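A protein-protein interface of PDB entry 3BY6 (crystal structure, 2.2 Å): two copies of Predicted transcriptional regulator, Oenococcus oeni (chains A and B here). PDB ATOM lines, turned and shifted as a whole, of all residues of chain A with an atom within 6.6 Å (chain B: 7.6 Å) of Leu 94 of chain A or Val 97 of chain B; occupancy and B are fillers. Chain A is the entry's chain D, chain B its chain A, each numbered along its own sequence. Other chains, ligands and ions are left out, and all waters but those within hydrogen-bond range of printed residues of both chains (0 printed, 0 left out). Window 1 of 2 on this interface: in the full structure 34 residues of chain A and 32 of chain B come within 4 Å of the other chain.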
ATOM      1  N   ARG A  89     -14.229  -8.991  12.558  1.00  0.00           N
ATOM      2  CA  ARG A  89     -14.156 -10.354  13.038  1.00  0.00           C
ATOM      3  C   ARG A  89     -14.513 -10.424  14.521  1.00  0.00           C
ATOM      4  O   ARG A  89     -15.368 -11.176  14.929  1.00  0.00           O
ATOM      5  CB  ARG A  89     -12.718 -10.883  12.827  1.00  0.00           C
ATOM      6  CG  ARG A  89     -12.473 -12.257  13.533  1.00  0.00           C
ATOM      7  CD  ARG A  89     -11.033 -12.752  13.317  1.00  0.00           C
ATOM      8  NE  ARG A  89     -10.055 -11.981  14.090  1.00  0.00           N
ATOM      9  CZ  ARG A  89      -9.949 -12.040  15.422  1.00  0.00           C
ATOM     10  NH1 ARG A  89     -10.746 -12.817  16.138  1.00  0.00           N
ATOM     11  NH2 ARG A  89      -9.061 -11.331  16.051  1.00  0.00           N
ATOM     12  N   LEU A  90     -13.849  -9.596  15.310  1.00  0.00           N
ATOM     13  CA  LEU A  90     -14.116  -9.468  16.737  1.00  0.00           C
ATOM     14  C   LEU A  90     -15.551  -8.980  17.018  1.00  0.00           C
ATOM     15  O   LEU A  90     -16.183  -9.366  17.997  1.00  0.00           O
ATOM     16  CB  LEU A  90     -13.078  -8.507  17.344  1.00  0.00           C
ATOM     17  CG  LEU A  90     -11.629  -9.074  17.328  1.00  0.00           C
ATOM     18  CD1 LEU A  90     -10.571  -8.068  17.704  1.00  0.00           C
ATOM     19  CD2 LEU A  90     -11.590 -10.293  18.219  1.00  0.00           C
ATOM     20  N   LEU A  91     -16.049  -8.101  16.168  1.00  0.00           N
ATOM     21  CA  LEU A  91     -17.406  -7.610  16.310  1.00  0.00           C
ATOM     22  C   LEU A  91     -18.394  -8.713  15.998  1.00  0.00           C
ATOM     23  O   LEU A  91     -19.428  -8.761  16.628  1.00  0.00           O
ATOM     24  CB  LEU A  91     -17.649  -6.432  15.390  1.00  0.00           C
ATOM     25  CG  LEU A  91     -17.134  -5.072  15.849  1.00  0.00           C
ATOM     26  CD1 LEU A  91     -17.342  -4.026  14.722  1.00  0.00           C
ATOM     27  CD2 LEU A  91     -17.895  -4.708  17.104  1.00  0.00           C
ATOM     28  N   ALA A  92     -18.071  -9.604  15.046  1.00  0.00           N
ATOM     29  CA  ALA A  92     -18.921 -10.765  14.756  1.00  0.00           C
ATOM     30  C   ALA A  92     -18.906 -11.739  15.952  1.00  0.00           C
ATOM     31  O   ALA A  92     -19.948 -12.228  16.408  1.00  0.00           O
ATOM     32  CB  ALA A  92     -18.477 -11.466  13.430  1.00  0.00           C
ATOM     33  N   ASP A  93     -17.714 -12.025  16.467  1.00  0.00           N
ATOM     34  CA  ASP A  93     -17.567 -12.781  17.701  1.00  0.00           C
ATOM     35  C   ASP A  93     -18.391 -12.108  18.822  1.00  0.00           C
ATOM     36  O   ASP A  93     -19.061 -12.795  19.611  1.00  0.00           O
ATOM     37  CB  ASP A  93     -16.104 -12.833  18.142  1.00  0.00           C
ATOM     38  CG  ASP A  93     -15.240 -13.711  17.258  1.00  0.00           C
ATOM     39  OD1 ASP A  93     -15.763 -14.396  16.362  1.00  0.00           O
ATOM     40  OD2 ASP A  93     -14.006 -13.691  17.442  1.00  0.00           O
ATOM     41  N   LEU A  94     -18.340 -10.780  18.902  1.00  0.00           N
ATOM     42  CA  LEU A  94     -19.086 -10.078  19.964  1.00  0.00           C
ATOM     43  C   LEU A  94     -20.599 -10.303  19.895  1.00  0.00           C
ATOM     44  O   LEU A  94     -21.193 -10.640  20.888  1.00  0.00           O
ATOM     45  CB  LEU A  94     -18.776  -8.572  20.000  1.00  0.00           C
ATOM     46  CG  LEU A  94     -19.614  -7.772  21.039  1.00  0.00           C
ATOM     47  CD1 LEU A  94     -19.315  -8.229  22.468  1.00  0.00           C
ATOM     48  CD2 LEU A  94     -19.398  -6.304  20.889  1.00  0.00           C
ATOM     49  N   SER A  95     -21.233 -10.135  18.735  1.00  0.00           N
ATOM     50  CA  SER A  95     -22.690 -10.391  18.634  1.00  0.00           C
ATOM     51  C   SER A  95     -23.059 -11.869  18.762  1.00  0.00           C
ATOM     52  O   SER A  95     -24.190 -12.186  19.119  1.00  0.00           O
ATOM     53  CB  SER A  95     -23.234  -9.885  17.307  1.00  0.00           C
ATOM     54  OG  SER A  95     -22.535 -10.565  16.312  1.00  0.00           O
ATOM     55  N   GLN A  96     -22.108 -12.740  18.422  1.00  0.00           N
ATOM     56  CA  GLN A  96     -22.231 -14.188  18.554  1.00  0.00           C
ATOM     57  C   GLN A  96     -22.355 -14.518  20.055  1.00  0.00           C
ATOM     58  O   GLN A  96     -23.379 -15.074  20.483  1.00  0.00           O
ATOM     59  CB  GLN A  96     -21.006 -14.849  17.889  1.00  0.00           C
ATOM     60  CG  GLN A  96     -20.745 -16.384  18.075  1.00  0.00           C
ATOM     61  CD  GLN A  96     -19.361 -16.829  17.415  1.00  0.00           C
ATOM     62  OE1 GLN A  96     -18.254 -16.588  17.973  1.00  0.00           O
ATOM     63  NE2 GLN A  96     -19.441 -17.447  16.220  1.00  0.00           N
ATOM     64  N   VAL A  97     -21.370 -14.096  20.862  1.00  0.00           N
ATOM     65  CA  VAL A  97     -21.437 -14.345  22.328  1.00  0.00           C
ATOM     66  C   VAL A  97     -22.696 -13.719  22.979  1.00  0.00           C
ATOM     67  O   VAL A  97     -23.357 -14.374  23.773  1.00  0.00           O
ATOM     68  CB  VAL A  97     -20.137 -13.983  23.092  1.00  0.00           C
ATOM     69  CG1 VAL A  97     -19.899 -12.486  23.128  1.00  0.00           C
ATOM     70  CG2 VAL A  97     -20.232 -14.503  24.509  1.00  0.00           C
ATOM     71  N   ILE A  98     -23.051 -12.496  22.625  1.00  0.00           N
ATOM     72  CA  ILE A  98     -24.273 -11.858  23.170  1.00  0.00           C
ATOM     73  C   ILE A  98     -25.544 -12.607  22.732  1.00  0.00           C
ATOM     74  O   ILE A  98     -26.488 -12.784  23.519  1.00  0.00           O
ATOM     75  CB  ILE A  98     -24.396 -10.394  22.738  1.00  0.00           C
ATOM     76  CG1 ILE A  98     -23.281  -9.545  23.345  1.00  0.00           C
ATOM     77  CG2 ILE A  98     -25.756  -9.835  23.092  1.00  0.00           C
ATOM     78  CD1 ILE A  98     -23.274  -8.092  22.896  1.00  0.00           C
ATOM     79  N   ALA A  99     -25.556 -13.065  21.478  1.00  0.00           N
ATOM     80  CA  ALA A  99     -26.652 -13.879  20.955  1.00  0.00           C
ATOM     81  C   ALA A  99     -26.854 -15.132  21.807  1.00  0.00           C
ATOM     82  O   ALA A  99     -27.960 -15.434  22.247  1.00  0.00           O
ATOM     83  CB  ALA A  99     -26.364 -14.285  19.478  1.00  0.00           C
ATOM     84  N   VAL A 115     -21.453  -5.754  30.680  1.00  0.00           N
ATOM     85  CA  VAL A 115     -20.511  -5.088  29.796  1.00  0.00           C
ATOM     86  C   VAL A 115     -19.953  -3.826  30.456  1.00  0.00           C
ATOM     87  O   VAL A 115     -18.753  -3.599  30.427  1.00  0.00           O
ATOM     88  CB  VAL A 115     -21.165  -4.815  28.412  1.00  0.00           C
ATOM     89  CG1 VAL A 115     -20.329  -3.861  27.571  1.00  0.00           C
ATOM     90  CG2 VAL A 115     -21.410  -6.150  27.668  1.00  0.00           C
ATOM     91  N   LEU B  90     -19.516 -18.559  28.830  1.00  0.00           N
ATOM     92  CA  LEU B  90     -19.924 -17.536  27.888  1.00  0.00           C
ATOM     93  C   LEU B  90     -19.473 -16.133  28.305  1.00  0.00           C
ATOM     94  O   LEU B  90     -19.089 -15.315  27.473  1.00  0.00           O
ATOM     95  CB  LEU B  90     -21.471 -17.555  27.785  1.00  0.00           C
ATOM     96  CG  LEU B  90     -22.207 -18.082  26.530  1.00  0.00           C
ATOM     97  CD1 LEU B  90     -21.311 -18.905  25.614  1.00  0.00           C
ATOM     98  CD2 LEU B  90     -23.498 -18.795  26.864  1.00  0.00           C
ATOM     99  N   LEU B  91     -19.597 -15.858  29.604  1.00  0.00           N
ATOM    100  CA  LEU B  91     -19.132 -14.630  30.212  1.00  0.00           C
ATOM    101  C   LEU B  91     -17.626 -14.523  30.117  1.00  0.00           C
ATOM    102  O   LEU B  91     -17.107 -13.438  29.912  1.00  0.00           O
ATOM    103  CB  LEU B  91     -19.562 -14.582  31.692  1.00  0.00           C
ATOM    104  CG  LEU B  91     -21.031 -14.252  31.998  1.00  0.00           C
ATOM    105  CD1 LEU B  91     -21.304 -14.472  33.481  1.00  0.00           C
ATOM    106  CD2 LEU B  91     -21.318 -12.835  31.550  1.00  0.00           C
ATOM    107  N   ALA B  92     -16.916 -15.622  30.281  1.00  0.00           N
ATOM    108  CA  ALA B  92     -15.478 -15.597  30.074  1.00  0.00           C
ATOM    109  C   ALA B  92     -15.163 -15.175  28.630  1.00  0.00           C
ATOM    110  O   ALA B  92     -14.209 -14.414  28.369  1.00  0.00           O
ATOM    111  CB  ALA B  92     -14.857 -16.970  30.396  1.00  0.00           C
ATOM    112  N   ASP B  93     -15.954 -15.692  27.681  1.00  0.00           N
ATOM    113  CA  ASP B  93     -15.749 -15.387  26.251  1.00  0.00           C
ATOM    114  C   ASP B  93     -16.074 -13.937  25.995  1.00  0.00           C
ATOM    115  O   ASP B  93     -15.320 -13.271  25.336  1.00  0.00           O
ATOM    116  CB  ASP B  93     -16.629 -16.257  25.339  1.00  0.00           C
ATOM    117  CG  ASP B  93     -16.262 -17.729  25.392  1.00  0.00           C
ATOM    118  OD1 ASP B  93     -15.152 -18.065  25.856  1.00  0.00           O
ATOM    119  OD2 ASP B  93     -17.108 -18.547  24.964  1.00  0.00           O
ATOM    120  N   LEU B  94     -17.221 -13.476  26.499  1.00  0.00           N
ATOM    121  CA  LEU B  94     -17.561 -12.049  26.450  1.00  0.00           C
ATOM    122  C   LEU B  94     -16.408 -11.165  26.916  1.00  0.00           C
ATOM    123  O   LEU B  94     -16.092 -10.175  26.275  1.00  0.00           O
ATOM    124  CB  LEU B  94     -18.801 -11.746  27.297  1.00  0.00           C
ATOM    125  CG  LEU B  94     -19.268 -10.298  27.386  1.00  0.00           C
ATOM    126  CD1 LEU B  94     -19.503  -9.682  25.947  1.00  0.00           C
ATOM    127  CD2 LEU B  94     -20.534 -10.210  28.266  1.00  0.00           C
ATOM    128  N   SER B  95     -15.826 -11.519  28.058  1.00  0.00           N
ATOM    129  CA  SER B  95     -14.756 -10.756  28.666  1.00  0.00           C
ATOM    130  C   SER B  95     -13.549 -10.710  27.741  1.00  0.00           C
ATOM    131  O   SER B  95     -12.972  -9.671  27.510  1.00  0.00           O
ATOM    132  CB  SER B  95     -14.380 -11.371  30.039  1.00  0.00           C
ATOM    133  OG  SER B  95     -13.241 -10.720  30.559  1.00  0.00           O
ATOM    134  N   GLN B  96     -13.195 -11.858  27.189  1.00  0.00           N
ATOM    135  CA  GLN B  96     -12.061 -11.982  26.279  1.00  0.00           C
ATOM    136  C   GLN B  96     -12.208 -11.226  24.933  1.00  0.00           C
ATOM    137  O   GLN B  96     -11.246 -10.651  24.452  1.00  0.00           O
ATOM    138  CB  GLN B  96     -11.843 -13.476  26.015  1.00  0.00           C
ATOM    139  CG  GLN B  96     -10.675 -13.849  25.104  1.00  0.00           C
ATOM    140  CD  GLN B  96     -10.938 -15.175  24.425  1.00  0.00           C
ATOM    141  OE1 GLN B  96     -11.234 -16.180  25.099  1.00  0.00           O
ATOM    142  NE2 GLN B  96     -10.907 -15.177  23.079  1.00  0.00           N
ATOM    143  N   VAL B  97     -13.382 -11.256  24.310  1.00  0.00           N
ATOM    144  CA  VAL B  97     -13.606 -10.510  23.062  1.00  0.00           C
ATOM    145  C   VAL B  97     -13.528  -8.996  23.307  1.00  0.00           C
ATOM    146  O   VAL B  97     -12.898  -8.261  22.535  1.00  0.00           O
ATOM    147  CB  VAL B  97     -14.972 -10.885  22.351  1.00  0.00           C
ATOM    148  CG1 VAL B  97     -16.156 -10.652  23.255  1.00  0.00           C
ATOM    149  CG2 VAL B  97     -15.155 -10.067  21.067  1.00  0.00           C
ATOM    150  N   ILE B  98     -14.141  -8.543  24.394  1.00  0.00           N
ATOM    151  CA  ILE B  98     -14.093  -7.142  24.744  1.00  0.00           C
ATOM    152  C   ILE B  98     -12.641  -6.717  25.023  1.00  0.00           C
ATOM    153  O   ILE B  98     -12.187  -5.675  24.522  1.00  0.00           O
ATOM    154  CB  ILE B  98     -14.943  -6.809  25.948  1.00  0.00           C
ATOM    155  CG1 ILE B  98     -16.423  -7.007  25.592  1.00  0.00           C
ATOM    156  CG2 ILE B  98     -14.633  -5.338  26.439  1.00  0.00           C
ATOM    157  CD1 ILE B  98     -17.388  -6.675  26.759  1.00  0.00           C
ATOM    158  N   ALA B  99     -11.900  -7.533  25.777  1.00  0.00           N
ATOM    159  CA  ALA B  99     -10.482  -7.210  25.981  1.00  0.00           C
ATOM    160  C   ALA B  99      -9.718  -7.056  24.658  1.00  0.00           C
ATOM    161  O   ALA B  99      -8.890  -6.180  24.520  1.00  0.00           O
ATOM    162  CB  ALA B  99      -9.804  -8.256  26.884  1.00  0.00           C
ATOM    163  N   GLU B 100      -9.994  -7.928  23.698  1.00  0.00           N
ATOM    164  CA  GLU B 100      -9.247  -7.966  22.447  1.00  0.00           C
ATOM    165  C   GLU B 100      -9.669  -6.805  21.535  1.00  0.00           C
ATOM    166  O   GLU B 100      -8.864  -6.242  20.799  1.00  0.00           O
ATOM    167  CB  GLU B 100      -9.401  -9.324  21.770  1.00  0.00           C
ATOM    168  CG  GLU B 100      -8.388  -9.521  20.636  1.00  0.00           C
ATOM    169  CD  GLU B 100      -8.480 -10.889  19.959  1.00  0.00           C
ATOM    170  OE1 GLU B 100      -9.074 -11.818  20.564  1.00  0.00           O
ATOM    171  OE2 GLU B 100      -7.972 -11.018  18.809  1.00  0.00           O
ATOM    172  N   LEU B 101     -10.939  -6.433  21.641  1.00  0.00           N
ATOM    173  CA  LEU B 101     -11.459  -5.218  21.044  1.00  0.00           C
ATOM    174  C   LEU B 101     -10.802  -3.958  21.612  1.00  0.00           C
ATOM    175  O   LEU B 101     -10.340  -3.137  20.841  1.00  0.00           O
ATOM    176  CB  LEU B 101     -12.988  -5.125  21.218  1.00  0.00           C
ATOM    177  CG  LEU B 101     -13.900  -5.843  20.217  1.00  0.00           C
ATOM    178  CD1 LEU B 101     -15.334  -5.685  20.639  1.00  0.00           C
ATOM    179  CD2 LEU B 101     -13.709  -5.336  18.771  1.00  0.00           C
ATOM    180  N   ILE B 102     -10.771  -3.747  22.927  1.00  0.00           N
ATOM    181  CA  ILE B 102     -10.122  -2.514  23.380  1.00  0.00           C
ATOM    182  C   ILE B 102      -8.639  -2.577  23.009  1.00  0.00           C
ATOM    183  O   ILE B 102      -8.053  -1.571  22.666  1.00  0.00           O
ATOM    184  CB  ILE B 102     -10.372  -2.074  24.892  1.00  0.00           C
ATOM    185  CG1 ILE B 102      -9.396  -2.747  25.834  1.00  0.00           C
ATOM    186  CG2 ILE B 102     -11.840  -2.201  25.336  1.00  0.00           C
ATOM    187  CD1 ILE B 102      -8.114  -1.899  25.999  1.00  0.00           C
ATOM    188  N   LYS B 103      -8.057  -3.764  23.004  1.00  0.00           N
ATOM    189  CA  LYS B 103      -6.670  -3.916  22.552  1.00  0.00           C
ATOM    190  C   LYS B 103      -6.492  -3.632  21.040  1.00  0.00           C
ATOM    191  O   LYS B 103      -5.427  -3.212  20.586  1.00  0.00           O
ATOM    192  CB  LYS B 103      -6.180  -5.319  22.899  1.00  0.00           C
ATOM    193  CG  LYS B 103      -4.688  -5.483  22.873  1.00  0.00           C
ATOM    194  CD  LYS B 103      -4.334  -6.923  23.194  1.00  0.00           C
ATOM    195  CE  LYS B 103      -2.878  -7.230  22.848  1.00  0.00           C
ATOM    196  NZ  LYS B 103      -2.571  -6.991  21.395  1.00  0.00           N
ATOM    197  N   SER B 104      -7.545  -3.844  20.261  1.00  0.00           N
ATOM    198  CA  SER B 104      -7.511  -3.577  18.827  1.00  0.00           C
ATOM    199  C   SER B 104      -7.654  -2.078  18.552  1.00  0.00           C
ATOM    200  O   SER B 104      -7.667  -1.649  17.387  1.00  0.00           O
ATOM    201  CB  SER B 104      -8.642  -4.327  18.108  1.00  0.00           C
ATOM    202  OG  SER B 104      -9.914  -3.708  18.322  1.00  0.00           O
ATOM    203  N   ARG B 110     -17.354   3.229  23.066  1.00  0.00           N
ATOM    204  CA  ARG B 110     -17.876   2.816  21.760  1.00  0.00           C
ATOM    205  C   ARG B 110     -18.303   1.362  21.781  1.00  0.00           C
ATOM    206  O   ARG B 110     -19.296   1.018  21.150  1.00  0.00           O
ATOM    207  CB  ARG B 110     -16.860   3.030  20.619  1.00  0.00           C
ATOM    208  CG  ARG B 110     -17.369   2.444  19.285  1.00  0.00           C
ATOM    209  CD  ARG B 110     -17.053   3.227  18.026  1.00  0.00           C
ATOM    210  NE  ARG B 110     -17.093   2.293  16.881  1.00  0.00           N
ATOM    211  CZ  ARG B 110     -16.033   1.838  16.189  1.00  0.00           C
ATOM    212  NH1 ARG B 110     -14.769   2.262  16.417  1.00  0.00           N
ATOM    213  NH2 ARG B 110     -16.252   0.942  15.232  1.00  0.00           N
ATOM    214  N   ILE B 111     -17.555   0.513  22.498  1.00  0.00           N
ATOM    215  CA  ILE B 111     -18.010  -0.854  22.778  1.00  0.00           C
ATOM    216  C   ILE B 111     -19.386  -0.784  23.480  1.00  0.00           C
ATOM    217  O   ILE B 111     -20.271  -1.565  23.172  1.00  0.00           O
ATOM    218  CB  ILE B 111     -16.953  -1.674  23.592  1.00  0.00           C
ATOM    219  CG1 ILE B 111     -15.649  -1.821  22.803  1.00  0.00           C
ATOM    220  CG2 ILE B 111     -17.500  -3.065  23.972  1.00  0.00           C
ATOM    221  CD1 ILE B 111     -14.524  -2.450  23.602  1.00  0.00           C
ATOM    222  N   LYS B 112     -19.577   0.163  24.402  1.00  0.00           N
ATOM    223  CA  LYS B 112     -20.866   0.317  25.067  1.00  0.00           C
ATOM    224  C   LYS B 112     -21.961   0.588  24.057  1.00  0.00           C
ATOM    225  O   LYS B 112     -22.994  -0.087  24.049  1.00  0.00           O
ATOM    226  CB  LYS B 112     -20.846   1.420  26.131  1.00  0.00           C
ATOM    227  CG  LYS B 112     -20.089   1.034  27.408  1.00  0.00           C
ATOM    228  CD  LYS B 112     -20.347   2.001  28.583  1.00  0.00           C
ATOM    229  CE  LYS B 112     -19.235   1.889  29.687  1.00  0.00           C
ATOM    230  NZ  LYS B 112     -17.989   2.716  29.311  1.00  0.00           N
ATOM    231  N   ILE B 114     -21.940   0.083  20.733  1.00  0.00           N
ATOM    232  CA  ILE B 114     -22.076  -1.061  19.845  1.00  0.00           C
ATOM    233  C   ILE B 114     -22.918  -2.149  20.479  1.00  0.00           C
ATOM    234  O   ILE B 114     -23.829  -2.676  19.862  1.00  0.00           O
ATOM    235  CB  ILE B 114     -20.662  -1.590  19.454  1.00  0.00           C
ATOM    236  CG1 ILE B 114     -19.938  -0.556  18.545  1.00  0.00           C
ATOM    237  CG2 ILE B 114     -20.734  -2.957  18.757  1.00  0.00           C
ATOM    238  CD1 ILE B 114     -18.447  -0.885  18.279  1.00  0.00           C
ATOM    239  N   VAL B 115     -22.605  -2.490  21.726  1.00  0.00           N
ATOM    240  CA  VAL B 115     -23.339  -3.476  22.468  1.00  0.00           C
ATOM    241  C   VAL B 115     -24.807  -3.060  22.604  1.00  0.00           C
ATOM    242  O   VAL B 115     -25.711  -3.874  22.416  1.00  0.00           O
ATOM    243  CB  VAL B 115     -22.659  -3.743  23.858  1.00  0.00           C
ATOM    244  CG1 VAL B 115     -23.577  -4.532  24.805  1.00  0.00           C
ATOM    245  CG2 VAL B 115     -21.288  -4.468  23.681  1.00  0.00           C
ATOM    246  N   ASN B 116     -25.055  -1.797  22.907  1.00  0.00           N
ATOM    247  CA  ASN B 116     -26.439  -1.314  22.990  1.00  0.00           C
ATOM    248  C   ASN B 116     -27.215  -1.463  21.663  1.00  0.00           C
ATOM    249  O   ASN B 116     -28.389  -1.843  21.665  1.00  0.00           O
ATOM    250  CB  ASN B 116     -26.458   0.143  23.441  1.00  0.00           C
ATOM    251  CG  ASN B 116     -27.855   0.623  23.773  1.00  0.00           C
ATOM    252  OD1 ASN B 116     -28.830  -0.120  23.625  1.00  0.00           O
ATOM    253  ND2 ASN B 116     -27.967   1.863  24.221  1.00  0.00           N
ATOM    254  N   ILE B 118     -26.373  -3.770  19.280  1.00  0.00           N
ATOM    255  CA  ILE B 118     -26.530  -5.224  19.123  1.00  0.00           C
ATOM    256  C   ILE B 118     -27.713  -5.752  19.923  1.00  0.00           C
ATOM    257  O   ILE B 118     -28.317  -6.737  19.516  1.00  0.00           O
ATOM    258  CB  ILE B 118     -25.277  -6.018  19.547  1.00  0.00           C
ATOM    259  CG1 ILE B 118     -24.102  -5.751  18.616  1.00  0.00           C
ATOM    260  CG2 ILE B 118     -25.567  -7.557  19.567  1.00  0.00           C
ATOM    261  CD1 ILE B 118     -22.763  -6.383  19.064  1.00  0.00           C
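OE2 of Glu 100 of chain B lies within salt-bridge range of NH2 of Arg 89 of chain A, 3.0 Å away.
The side-chain hydroxyl of Ser 104 of chain B is in hydrogen-bond range of the backbone carbonyl oxygen of Leu 101 of chain B (2.6 Å).
NH1 of Arg 89 of chain A is in salt-bridge range of OD2 of Asp 93 of chain A (3.6 Å).
The backbone carbonyl oxygen (O) of Ala 92 of chain A lies within hydrogen-bond range of the side-chain hydroxyl (OG) of Ser 95 of chain A, 3.1 Å away.
Leu 90 of chain A touches Val 97 of chain B (O to CG2, 3.3 Å).
CD2 of Leu 90 of chain A touches CD of Glu 100 of chain B (3.6 Å).
Leu 101 of chain B touches Leu 90 of chain A (CD2 to CB, 3.5 Å).
CD2 of Leu 91 of chain A touches CG2 of Ile 114 of chain B, at 3.7 Å.
Leu 94 of chain A touches Leu 94 of chain B.
N of Leu 94 of chain A touches CG2 of Val 97 of chain B, 3.9 Å away.
Val 115 of chain B touches Leu 94 of chain A (CG2 to CD2, 3.8 Å).
CD1 of Ile 118 of chain B touches CB of Ser 95 of chain A, 3.9 Å away.
Leu 90 of chain B touches Val 97 of chain A (O to CG2, 3.3 Å).
Val 97 of chain A touches Leu 94 of chain B (CG2 to N, 3.8 Å).
Of chain B, only Leu 94, Val 97, Val 115 and Ile 118 come within 4 Å of Leu 94 of chain A.
Of chain A, only Leu 90 (3.3 Å) and Leu 94 (3.9 Å) come within 4 Å of Val 97 of chain B.
Of the printed residues of chain B, Leu 90 of chain A touches Val 97, Glu 100 and Leu 101.
Printed residues of chain A within 4 Å of Leu 94 of chain B: Leu 94 (3.8 Å) and Val 97 (3.8 Å).
Of the printed residues of chain A, Leu 101 of chain B touches Leu 90.
Of the printed residues of chain B, Leu 91 of chain A touches Ile 114.
Ala 99 of chain A touches none of the printed residues of chain B.
The nearest residue of chain B that does not touch Leu 94 of chain A is Leu 101 of chain B (4.1 Å).
The nearest residue of chain A that does not touch Val 97 of chain B is Asp 93 of chain A (4.1 Å).
The nearest printed residue of chain B that does not touch Ser 95 of chain A is Val 97 of chain B (6.5 Å).
Hydrophobic or aromatic side chains of chain A that line the printed part of chain B: Leu 90, Leu 91, Leu 94, Val 97 and Val 115.
Hydrophobic or aromatic side chains of chain B within 4 Å of the printed part of chain A: Leu 94, Val 97, Leu 101, Ile 114, Val 115 and Ile 118.
Along chain B the printed residues that touch a printed residue of chain A span positions 90 to 118.
Among the printed residues, 13 pairs touch across the chains.
Among the printed residues, Asp or Glu carboxylates within 4 Å of a Lys or Arg side-chain nitrogen of the other chain: Arg 89 of chain A with Glu 100 of chain B.
Leu 90 of chain A touches Val 97 of chain B, and with the chains exchanged Val 97 of chain A touches Leu 90 of chain B.
Leu 94 of chain A touches Val 97 of chain B, and with the chains exchanged Val 97 of chain A touches Leu 94 of chain B.
Leu 94 of chain A touches Val 115 of chain B, but with the chains exchanged Val 115 of chain A does not touch Leu 94 of chain B (4.2 Å).
Val 115 of chain B touches its own counterpart, Val 115 of chain A.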
